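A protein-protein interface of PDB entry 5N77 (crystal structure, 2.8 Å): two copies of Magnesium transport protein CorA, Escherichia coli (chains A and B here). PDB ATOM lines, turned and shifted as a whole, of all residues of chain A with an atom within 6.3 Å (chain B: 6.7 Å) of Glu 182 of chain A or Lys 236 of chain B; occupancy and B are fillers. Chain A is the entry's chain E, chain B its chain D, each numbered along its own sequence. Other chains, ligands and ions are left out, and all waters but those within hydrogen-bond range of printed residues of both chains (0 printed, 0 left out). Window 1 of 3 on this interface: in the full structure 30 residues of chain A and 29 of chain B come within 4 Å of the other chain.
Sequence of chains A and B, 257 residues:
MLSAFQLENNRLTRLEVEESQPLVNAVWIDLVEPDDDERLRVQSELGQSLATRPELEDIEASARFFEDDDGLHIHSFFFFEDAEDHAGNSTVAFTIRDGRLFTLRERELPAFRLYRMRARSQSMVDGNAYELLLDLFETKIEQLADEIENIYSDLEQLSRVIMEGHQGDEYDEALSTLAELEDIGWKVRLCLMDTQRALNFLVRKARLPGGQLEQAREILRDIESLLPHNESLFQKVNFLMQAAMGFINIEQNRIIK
The side-chain amino group of Lys 187 of chain A lies within salt-bridge range of the side-chain carboxylate of Glu 156 of chain B. The side-chain hydroxyl (OG) of Ser 232 of chain B lies within hydrogen-bond range of the indole nitrogen (NE1) of Trp 186 of chain A, 3.1 Å away. OE1 of Glu 182 of chain A lies within salt-bridge range of NZ of Lys 236 of chain B, 2.9 Å away. The side-chain amino group (NZ) of Lys 236 of chain B is in salt-bridge range of the side-chain carboxylate (OD1) of Asp 183 of chain A, 2.7 Å away.
The side-chain amino group (NZ) of Lys 187 of chain A lies within salt-bridge range of the side-chain carboxylate (OD2) of Asp 183 of chain A, 2.8 Å away. ND2 of Asn 238 of chain A sits at hydrogen-bond distance from O of Phe 234 of chain A (3.1 Å).
Among the printed residues, pairs that only touch across the chains: Asn 238 of chain A with Phe 239 of chain B, Val 237 of chain A with Phe 239 of chain B, Glu 182 of chain A with Phe 239 of chain B, Trp 186 of chain A with Lys 236 of chain B and Ala 179 of chain A with Phe 239 of chain B.
Ile 151 of chain A touches none of the printed residues of chain B. Printed residues of chain B within 4 Å of Ala 179 of chain A: Phe 239 (3.9 Å). Glu 182 of chain A touches just these residues of chain B: Lys 236 and Phe 239. Of the printed residues of chain B, Asp 183 of chain A touches Lys 236 (2.7 Å). Printed residues of chain B within 4 Å of Val 237 of chain A: Phe 239. Of the printed residues of chain A, Glu 156 of chain B touches Lys 187. Printed residues of chain A within 4 Å of Ser 232 of chain B: Trp 186 (3.1 Å). Gln 235 of chain B touches none of the printed residues of chain A. Lys 236 of chain B touches just these residues of chain A: Glu 182 (2.9 Å), Asp 183 (2.7 Å) and Trp 186 (3.8 Å). The nearest residue of chain A that does not touch Lys 236 of chain B is Ala 179 of chain A (4.8 Å). The nearest printed residue of chain B that does not touch Trp 186 of chain A is Leu 233 of chain B (4.3 Å).
Of the 15 printed residues of chain A, 7 touch a printed residue of chain B. Hydrophobic or aromatic side chains of chain A that line the printed part of chain B: Ala 179, Trp 186 and Val 237. Hydrophobic or aromatic side chains of chain B that line the printed part of chain A: Phe 239. Along chain B the printed residues that touch a printed residue of chain A span positions 156 to 239. Among the printed residues, 9 pairs touch across the chains.
4 positions are printed for both chains. Of the 9 pairs that touch across the chains among the printed residues, none has its exchanged pair printed and touching as well.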
ATOM      1  N   ILE A 151      27.170 -19.819  29.533  1.00  0.00           N
ATOM      2  CA  ILE A 151      26.783 -19.231  28.276  1.00  0.00           C
ATOM      3  C   ILE A 151      27.929 -18.364  27.765  1.00  0.00           C
ATOM      4  O   ILE A 151      28.266 -18.419  26.584  1.00  0.00           O
ATOM      5  CB  ILE A 151      25.521 -18.390  28.383  1.00  0.00           C
ATOM      6  CG1 ILE A 151      24.337 -19.244  28.816  1.00  0.00           C
ATOM      7  CG2 ILE A 151      25.170 -17.810  27.033  1.00  0.00           C
ATOM      8  CD1 ILE A 151      23.089 -18.432  29.094  1.00  0.00           C
ATOM      9  N   THR A 177      23.860 -24.216  17.745  1.00  0.00           N
ATOM     10  CA  THR A 177      24.435 -23.896  19.058  1.00  0.00           C
ATOM     11  C   THR A 177      24.017 -22.497  19.505  1.00  0.00           C
ATOM     12  O   THR A 177      23.592 -22.303  20.637  1.00  0.00           O
ATOM     13  CB  THR A 177      25.978 -24.034  19.079  1.00  0.00           C
ATOM     14  OG1 THR A 177      26.358 -25.294  18.507  1.00  0.00           O
ATOM     15  CG2 THR A 177      26.504 -23.978  20.494  1.00  0.00           C
ATOM     16  N   LEU A 178      24.143 -21.522  18.625  1.00  0.00           N
ATOM     17  CA  LEU A 178      23.647 -20.185  18.928  1.00  0.00           C
ATOM     18  C   LEU A 178      22.239 -20.178  19.478  1.00  0.00           C
ATOM     19  O   LEU A 178      21.938 -19.480  20.447  1.00  0.00           O
ATOM     20  CB  LEU A 178      23.577 -19.332  17.681  1.00  0.00           C
ATOM     21  CG  LEU A 178      24.576 -18.221  17.543  1.00  0.00           C
ATOM     22  CD1 LEU A 178      24.021 -17.318  16.469  1.00  0.00           C
ATOM     23  CD2 LEU A 178      24.788 -17.434  18.819  1.00  0.00           C
ATOM     24  N   ALA A 179      21.366 -20.924  18.814  1.00  0.00           N
ATOM     25  CA  ALA A 179      19.964 -20.972  19.187  1.00  0.00           C
ATOM     26  C   ALA A 179      19.749 -21.715  20.521  1.00  0.00           C
ATOM     27  O   ALA A 179      18.823 -21.404  21.247  1.00  0.00           O
ATOM     28  CB  ALA A 179      19.163 -21.611  18.076  1.00  0.00           C
ATOM     29  N   GLU A 180      20.602 -22.691  20.819  1.00  0.00           N
ATOM     30  CA  GLU A 180      20.599 -23.345  22.126  1.00  0.00           C
ATOM     31  C   GLU A 180      20.997 -22.336  23.240  1.00  0.00           C
ATOM     32  O   GLU A 180      20.433 -22.326  24.329  1.00  0.00           O
ATOM     33  CB  GLU A 180      21.535 -24.586  22.146  1.00  0.00           C
ATOM     34  CG  GLU A 180      20.925 -25.946  21.706  1.00  0.00           C
ATOM     35  CD  GLU A 180      21.963 -27.057  21.332  1.00  0.00           C
ATOM     36  OE1 GLU A 180      23.084 -26.715  20.874  1.00  0.00           O
ATOM     37  OE2 GLU A 180      21.671 -28.297  21.472  1.00  0.00           O
ATOM     38  N   LEU A 181      22.000 -21.504  22.969  1.00  0.00           N
ATOM     39  CA  LEU A 181      22.476 -20.543  23.963  1.00  0.00           C
ATOM     40  C   LEU A 181      21.466 -19.419  24.167  1.00  0.00           C
ATOM     41  O   LEU A 181      21.268 -18.959  25.287  1.00  0.00           O
ATOM     42  CB  LEU A 181      23.865 -20.005  23.595  1.00  0.00           C
ATOM     43  CG  LEU A 181      24.976 -21.082  23.577  1.00  0.00           C
ATOM     44  CD1 LEU A 181      26.330 -20.548  23.132  1.00  0.00           C
ATOM     45  CD2 LEU A 181      25.132 -21.719  24.944  1.00  0.00           C
ATOM     46  N   GLU A 182      20.825 -18.991  23.085  1.00  0.00           N
ATOM     47  CA  GLU A 182      19.788 -17.978  23.179  1.00  0.00           C
ATOM     48  C   GLU A 182      18.705 -18.503  24.086  1.00  0.00           C
ATOM     49  O   GLU A 182      18.252 -17.810  24.981  1.00  0.00           O
ATOM     50  CB  GLU A 182      19.192 -17.641  21.811  1.00  0.00           C
ATOM     51  CG  GLU A 182      18.359 -16.361  21.772  1.00  0.00           C
ATOM     52  CD  GLU A 182      16.886 -16.544  22.142  1.00  0.00           C
ATOM     53  OE1 GLU A 182      16.393 -17.701  22.139  1.00  0.00           O
ATOM     54  OE2 GLU A 182      16.217 -15.512  22.445  1.00  0.00           O
ATOM     55  N   ASP A 183      18.299 -19.744  23.859  1.00  0.00           N
ATOM     56  CA  ASP A 183      17.203 -20.328  24.605  1.00  0.00           C
ATOM     57  C   ASP A 183      17.516 -20.468  26.092  1.00  0.00           C
ATOM     58  O   ASP A 183      16.655 -20.281  26.937  1.00  0.00           O
ATOM     59  CB  ASP A 183      16.863 -21.690  24.036  1.00  0.00           C
ATOM     60  CG  ASP A 183      15.598 -22.254  24.614  1.00  0.00           C
ATOM     61  OD1 ASP A 183      14.532 -21.625  24.388  1.00  0.00           O
ATOM     62  OD2 ASP A 183      15.679 -23.323  25.285  1.00  0.00           O
ATOM     63  N   ILE A 184      18.735 -20.859  26.412  1.00  0.00           N
ATOM     64  CA  ILE A 184      19.110 -20.999  27.803  1.00  0.00           C
ATOM     65  C   ILE A 184      18.985 -19.623  28.444  1.00  0.00           C
ATOM     66  O   ILE A 184      18.325 -19.472  29.451  1.00  0.00           O
ATOM     67  CB  ILE A 184      20.531 -21.582  27.964  1.00  0.00           C
ATOM     68  CG1 ILE A 184      20.540 -23.022  27.491  1.00  0.00           C
ATOM     69  CG2 ILE A 184      20.945 -21.613  29.424  1.00  0.00           C
ATOM     70  CD1 ILE A 184      21.913 -23.536  27.202  1.00  0.00           C
ATOM     71  N   GLY A 185      19.640 -18.630  27.860  1.00  0.00           N
ATOM     72  CA  GLY A 185      19.627 -17.270  28.405  1.00  0.00           C
ATOM     73  C   GLY A 185      18.232 -16.726  28.583  1.00  0.00           C
ATOM     74  O   GLY A 185      17.924 -16.077  29.573  1.00  0.00           O
ATOM     75  N   TRP A 186      17.376 -17.054  27.637  1.00  0.00           N
ATOM     76  CA  TRP A 186      15.976 -16.645  27.653  1.00  0.00           C
ATOM     77  C   TRP A 186      15.254 -17.241  28.843  1.00  0.00           C
ATOM     78  O   TRP A 186      14.539 -16.548  29.535  1.00  0.00           O
ATOM     79  CB  TRP A 186      15.305 -17.123  26.364  1.00  0.00           C
ATOM     80  CG  TRP A 186      13.938 -16.630  26.110  1.00  0.00           C
ATOM     81  CD1 TRP A 186      13.554 -15.341  25.931  1.00  0.00           C
ATOM     82  CD2 TRP A 186      12.777 -17.425  25.955  1.00  0.00           C
ATOM     83  NE1 TRP A 186      12.210 -15.280  25.714  1.00  0.00           N
ATOM     84  CE2 TRP A 186      11.708 -16.554  25.719  1.00  0.00           C
ATOM     85  CE3 TRP A 186      12.535 -18.805  25.989  1.00  0.00           C
ATOM     86  CZ2 TRP A 186      10.418 -17.010  25.505  1.00  0.00           C
ATOM     87  CZ3 TRP A 186      11.247 -19.256  25.800  1.00  0.00           C
ATOM     88  CH2 TRP A 186      10.206 -18.361  25.552  1.00  0.00           C
ATOM     89  N   LYS A 187      15.455 -18.527  29.060  1.00  0.00           N
ATOM     90  CA  LYS A 187      14.824 -19.236  30.152  1.00  0.00           C
ATOM     91  C   LYS A 187      15.410 -18.881  31.511  1.00  0.00           C
ATOM     92  O   LYS A 187      14.712 -18.882  32.508  1.00  0.00           O
ATOM     93  CB  LYS A 187      14.888 -20.741  29.912  1.00  0.00           C
ATOM     94  CG  LYS A 187      13.750 -21.186  29.012  1.00  0.00           C
ATOM     95  CD  LYS A 187      14.029 -22.464  28.268  1.00  0.00           C
ATOM     96  CE  LYS A 187      12.964 -22.698  27.206  1.00  0.00           C
ATOM     97  NZ  LYS A 187      13.205 -23.991  26.499  1.00  0.00           N
ATOM     98  N   PHE A 234      22.121 -11.421  24.914  1.00  0.00           N
ATOM     99  CA  PHE A 234      21.194 -11.343  23.765  1.00  0.00           C
ATOM    100  C   PHE A 234      21.742 -10.454  22.664  1.00  0.00           C
ATOM    101  O   PHE A 234      21.581 -10.780  21.506  1.00  0.00           O
ATOM    102  CB  PHE A 234      19.772 -10.911  24.150  1.00  0.00           C
ATOM    103  CG  PHE A 234      19.059 -11.910  25.010  1.00  0.00           C
ATOM    104  CD1 PHE A 234      18.906 -13.230  24.600  1.00  0.00           C
ATOM    105  CD2 PHE A 234      18.558 -11.538  26.263  1.00  0.00           C
ATOM    106  CE1 PHE A 234      18.255 -14.151  25.418  1.00  0.00           C
ATOM    107  CE2 PHE A 234      17.906 -12.451  27.085  1.00  0.00           C
ATOM    108  CZ  PHE A 234      17.754 -13.760  26.661  1.00  0.00           C
ATOM    109  N   VAL A 237      24.542 -12.562  20.947  1.00  0.00           N
ATOM    110  CA  VAL A 237      23.873 -13.592  20.172  1.00  0.00           C
ATOM    111  C   VAL A 237      23.237 -13.075  18.874  1.00  0.00           C
ATOM    112  O   VAL A 237      23.364 -13.705  17.845  1.00  0.00           O
ATOM    113  CB  VAL A 237      22.792 -14.285  21.003  1.00  0.00           C
ATOM    114  CG1 VAL A 237      21.814 -15.046  20.106  1.00  0.00           C
ATOM    115  CG2 VAL A 237      23.472 -15.225  21.972  1.00  0.00           C
ATOM    116  N   ASN A 238      22.520 -11.958  18.954  1.00  0.00           N
ATOM    117  CA  ASN A 238      21.832 -11.399  17.794  1.00  0.00           C
ATOM    118  C   ASN A 238      22.792 -10.869  16.774  1.00  0.00           C
ATOM    119  O   ASN A 238      22.524 -10.938  15.574  1.00  0.00           O
ATOM    120  CB  ASN A 238      20.874 -10.279  18.188  1.00  0.00           C
ATOM    121  CG  ASN A 238      19.629 -10.797  18.883  1.00  0.00           C
ATOM    122  OD1 ASN A 238      19.124 -11.886  18.583  1.00  0.00           O
ATOM    123  ND2 ASN A 238      19.121 -10.019  19.814  1.00  0.00           N
ATOM    124  N   LEU B 155       5.301 -22.221  21.113  1.00  0.00           N
ATOM    125  CA  LEU B 155       6.560 -21.638  20.675  1.00  0.00           C
ATOM    126  C   LEU B 155       7.721 -22.563  21.018  1.00  0.00           C
ATOM    127  O   LEU B 155       8.741 -22.598  20.334  1.00  0.00           O
ATOM    128  CB  LEU B 155       6.751 -20.303  21.352  1.00  0.00           C
ATOM    129  CG  LEU B 155       7.775 -19.353  20.780  1.00  0.00           C
ATOM    130  CD1 LEU B 155       7.425 -18.979  19.358  1.00  0.00           C
ATOM    131  CD2 LEU B 155       7.805 -18.093  21.622  1.00  0.00           C
ATOM    132  N   GLU B 156       7.546 -23.313  22.091  1.00  0.00           N
ATOM    133  CA  GLU B 156       8.529 -24.288  22.541  1.00  0.00           C
ATOM    134  C   GLU B 156       8.629 -25.406  21.522  1.00  0.00           C
ATOM    135  O   GLU B 156       9.719 -25.810  21.165  1.00  0.00           O
ATOM    136  CB  GLU B 156       8.118 -24.813  23.926  1.00  0.00           C
ATOM    137  CG  GLU B 156       9.069 -25.779  24.609  1.00  0.00           C
ATOM    138  CD  GLU B 156      10.481 -25.245  24.780  1.00  0.00           C
ATOM    139  OE1 GLU B 156      10.654 -24.057  25.182  1.00  0.00           O
ATOM    140  OE2 GLU B 156      11.425 -26.039  24.527  1.00  0.00           O
ATOM    141  N   SER B 159      10.003 -24.073  18.246  1.00  0.00           N
ATOM    142  CA  SER B 159      11.426 -23.819  18.374  1.00  0.00           C
ATOM    143  C   SER B 159      12.276 -25.009  17.931  1.00  0.00           C
ATOM    144  O   SER B 159      13.310 -24.860  17.279  1.00  0.00           O
ATOM    145  CB  SER B 159      11.761 -23.492  19.812  1.00  0.00           C
ATOM    146  OG  SER B 159      13.069 -22.969  19.881  1.00  0.00           O
ATOM    147  N   LEU B 178       4.906 -19.293  13.332  1.00  0.00           N
ATOM    148  CA  LEU B 178       5.535 -18.143  13.961  1.00  0.00           C
ATOM    149  C   LEU B 178       4.726 -16.866  13.853  1.00  0.00           C
ATOM    150  O   LEU B 178       4.587 -16.120  14.820  1.00  0.00           O
ATOM    151  CB  LEU B 178       6.854 -17.834  13.309  1.00  0.00           C
ATOM    152  CG  LEU B 178       8.107 -18.149  14.087  1.00  0.00           C
ATOM    153  CD1 LEU B 178       9.204 -17.363  13.399  1.00  0.00           C
ATOM    154  CD2 LEU B 178       8.028 -17.762  15.548  1.00  0.00           C
ATOM    155  N   GLU B 231       6.315  -9.203  26.127  1.00  0.00           N
ATOM    156  CA  GLU B 231       7.484  -8.575  25.486  1.00  0.00           C
ATOM    157  C   GLU B 231       8.600  -9.603  25.264  1.00  0.00           C
ATOM    158  O   GLU B 231       9.377  -9.530  24.330  1.00  0.00           O
ATOM    159  CB  GLU B 231       8.015  -7.398  26.335  1.00  0.00           C
ATOM    160  CG  GLU B 231       8.377  -6.160  25.521  1.00  0.00           C
ATOM    161  CD  GLU B 231       7.185  -5.594  24.740  1.00  0.00           C
ATOM    162  OE1 GLU B 231       6.016  -5.717  25.205  1.00  0.00           O
ATOM    163  OE2 GLU B 231       7.408  -5.024  23.643  1.00  0.00           O
ATOM    164  N   SER B 232       8.658 -10.559  26.171  1.00  0.00           N
ATOM    165  CA  SER B 232       9.618 -11.614  26.124  1.00  0.00           C
ATOM    166  C   SER B 232       9.351 -12.512  24.925  1.00  0.00           C
ATOM    167  O   SER B 232      10.275 -12.955  24.275  1.00  0.00           O
ATOM    168  CB  SER B 232       9.529 -12.406  27.420  1.00  0.00           C
ATOM    169  OG  SER B 232      10.506 -13.416  27.440  1.00  0.00           O
ATOM    170  N   LEU B 233       8.081 -12.803  24.652  1.00  0.00           N
ATOM    171  CA  LEU B 233       7.720 -13.625  23.509  1.00  0.00           C
ATOM    172  C   LEU B 233       8.131 -12.962  22.211  1.00  0.00           C
ATOM    173  O   LEU B 233       8.623 -13.646  21.323  1.00  0.00           O
ATOM    174  CB  LEU B 233       6.240 -13.909  23.476  1.00  0.00           C
ATOM    175  CG  LEU B 233       5.715 -14.717  24.651  1.00  0.00           C
ATOM    176  CD1 LEU B 233       4.201 -14.724  24.606  1.00  0.00           C
ATOM    177  CD2 LEU B 233       6.243 -16.133  24.660  1.00  0.00           C
ATOM    178  N   PHE B 234       7.978 -11.646  22.094  1.00  0.00           N
ATOM    179  CA  PHE B 234       8.416 -10.954  20.865  1.00  0.00           C
ATOM    180  C   PHE B 234       9.900 -11.118  20.584  1.00  0.00           C
ATOM    181  O   PHE B 234      10.273 -11.293  19.434  1.00  0.00           O
ATOM    182  CB  PHE B 234       8.041  -9.456  20.833  1.00  0.00           C
ATOM    183  CG  PHE B 234       6.561  -9.217  20.815  1.00  0.00           C
ATOM    184  CD1 PHE B 234       5.759  -9.808  19.825  1.00  0.00           C
ATOM    185  CD2 PHE B 234       5.945  -8.439  21.800  1.00  0.00           C
ATOM    186  CE1 PHE B 234       4.380  -9.613  19.824  1.00  0.00           C
ATOM    187  CE2 PHE B 234       4.569  -8.239  21.803  1.00  0.00           C
ATOM    188  CZ  PHE B 234       3.789  -8.828  20.818  1.00  0.00           C
ATOM    189  N   GLN B 235      10.742 -11.084  21.603  1.00  0.00           N
ATOM    190  CA  GLN B 235      12.175 -11.281  21.398  1.00  0.00           C
ATOM    191  C   GLN B 235      12.479 -12.643  20.809  1.00  0.00           C
ATOM    192  O   GLN B 235      13.272 -12.764  19.894  1.00  0.00           O
ATOM    193  CB  GLN B 235      12.935 -11.230  22.706  1.00  0.00           C
ATOM    194  CG  GLN B 235      13.142  -9.853  23.288  1.00  0.00           C
ATOM    195  CD  GLN B 235      14.479  -9.760  24.000  1.00  0.00           C
ATOM    196  OE1 GLN B 235      15.303 -10.703  23.965  1.00  0.00           O
ATOM    197  NE2 GLN B 235      14.721  -8.613  24.630  1.00  0.00           N
ATOM    198  N   LYS B 236      11.871 -13.666  21.401  1.00  0.00           N
ATOM    199  CA  LYS B 236      12.024 -15.062  20.979  1.00  0.00           C
ATOM    200  C   LYS B 236      11.528 -15.216  19.560  1.00  0.00           C
ATOM    201  O   LYS B 236      12.208 -15.742  18.726  1.00  0.00           O
ATOM    202  CB  LYS B 236      11.236 -15.995  21.911  1.00  0.00           C
ATOM    203  CG  LYS B 236      11.441 -17.481  21.674  1.00  0.00           C
ATOM    204  CD  LYS B 236      12.836 -17.909  22.077  1.00  0.00           C
ATOM    205  CE  LYS B 236      13.006 -19.418  21.980  1.00  0.00           C
ATOM    206  NZ  LYS B 236      14.395 -19.829  22.322  1.00  0.00           N
ATOM    207  N   VAL B 237      10.337 -14.732  19.304  1.00  0.00           N
ATOM    208  CA  VAL B 237       9.777 -14.823  17.980  1.00  0.00           C
ATOM    209  C   VAL B 237      10.672 -14.200  16.948  1.00  0.00           C
ATOM    210  O   VAL B 237      10.847 -14.779  15.868  1.00  0.00           O
ATOM    211  CB  VAL B 237       8.413 -14.157  17.916  1.00  0.00           C
ATOM    212  CG1 VAL B 237       8.029 -13.829  16.479  1.00  0.00           C
ATOM    213  CG2 VAL B 237       7.400 -15.092  18.541  1.00  0.00           C
ATOM    214  N   ASN B 238      11.209 -13.020  17.246  1.00  0.00           N
ATOM    215  CA  ASN B 238      12.071 -12.304  16.279  1.00  0.00           C
ATOM    216  C   ASN B 238      13.381 -12.996  16.047  1.00  0.00           C
ATOM    217  O   ASN B 238      13.911 -12.962  14.945  1.00  0.00           O
ATOM    218  CB  ASN B 238      12.343 -10.864  16.711  1.00  0.00           C
ATOM    219  CG  ASN B 238      11.125  -9.947  16.530  1.00  0.00           C
ATOM    220  OD1 ASN B 238      10.309 -10.121  15.613  1.00  0.00           O
ATOM    221  ND2 ASN B 238      10.975  -9.001  17.441  1.00  0.00           N
ATOM    222  N   PHE B 239      13.906 -13.612  17.105  1.00  0.00           N
ATOM    223  CA  PHE B 239      15.123 -14.341  17.015  1.00  0.00           C
ATOM    224  C   PHE B 239      14.893 -15.606  16.185  1.00  0.00           C
ATOM    225  O   PHE B 239      15.718 -15.964  15.338  1.00  0.00           O
ATOM    226  CB  PHE B 239      15.654 -14.721  18.379  1.00  0.00           C
ATOM    227  CG  PHE B 239      16.799 -15.676  18.301  1.00  0.00           C
ATOM    228  CD1 PHE B 239      18.051 -15.225  17.954  1.00  0.00           C
ATOM    229  CD2 PHE B 239      16.612 -17.022  18.468  1.00  0.00           C
ATOM    230  CE1 PHE B 239      19.107 -16.094  17.825  1.00  0.00           C
ATOM    231  CE2 PHE B 239      17.668 -17.913  18.343  1.00  0.00           C
ATOM    232  CZ  PHE B 239      18.915 -17.447  18.012  1.00  0.00           C
ATOM    233  N   LEU B 240      13.787 -16.289  16.426  1.00  0.00           N
ATOM    234  CA  LEU B 240      13.465 -17.505  15.674  1.00  0.00           C
ATOM    235  C   LEU B 240      13.327 -17.207  14.178  1.00  0.00           C
ATOM    236  O   LEU B 240      13.799 -17.985  13.340  1.00  0.00           O
ATOM    237  CB  LEU B 240      12.190 -18.153  16.179  1.00  0.00           C
ATOM    238  CG  LEU B 240      12.334 -19.183  17.307  1.00  0.00           C
ATOM    239  CD1 LEU B 240      12.753 -18.524  18.600  1.00  0.00           C
ATOM    240  CD2 LEU B 240      10.962 -19.797  17.553  1.00  0.00           C
ATOM    241  N   MET B 241      12.693 -16.088  13.857  1.00  0.00           N
ATOM    242  CA  MET B 241      12.569 -15.633  12.494  1.00  0.00           C
ATOM    243  C   MET B 241      13.949 -15.480  11.853  1.00  0.00           C
ATOM    244  O   MET B 241      14.188 -15.892  10.732  1.00  0.00           O
ATOM    245  CB  MET B 241      11.831 -14.300  12.494  1.00  0.00           C
ATOM    246  CG  MET B 241      11.510 -13.719  11.127  1.00  0.00           C
ATOM    247  SD  MET B 241      10.518 -14.822  10.104  1.00  0.00           S
ATOM    248  CE  MET B 241       9.028 -14.714  11.092  1.00  0.00           C
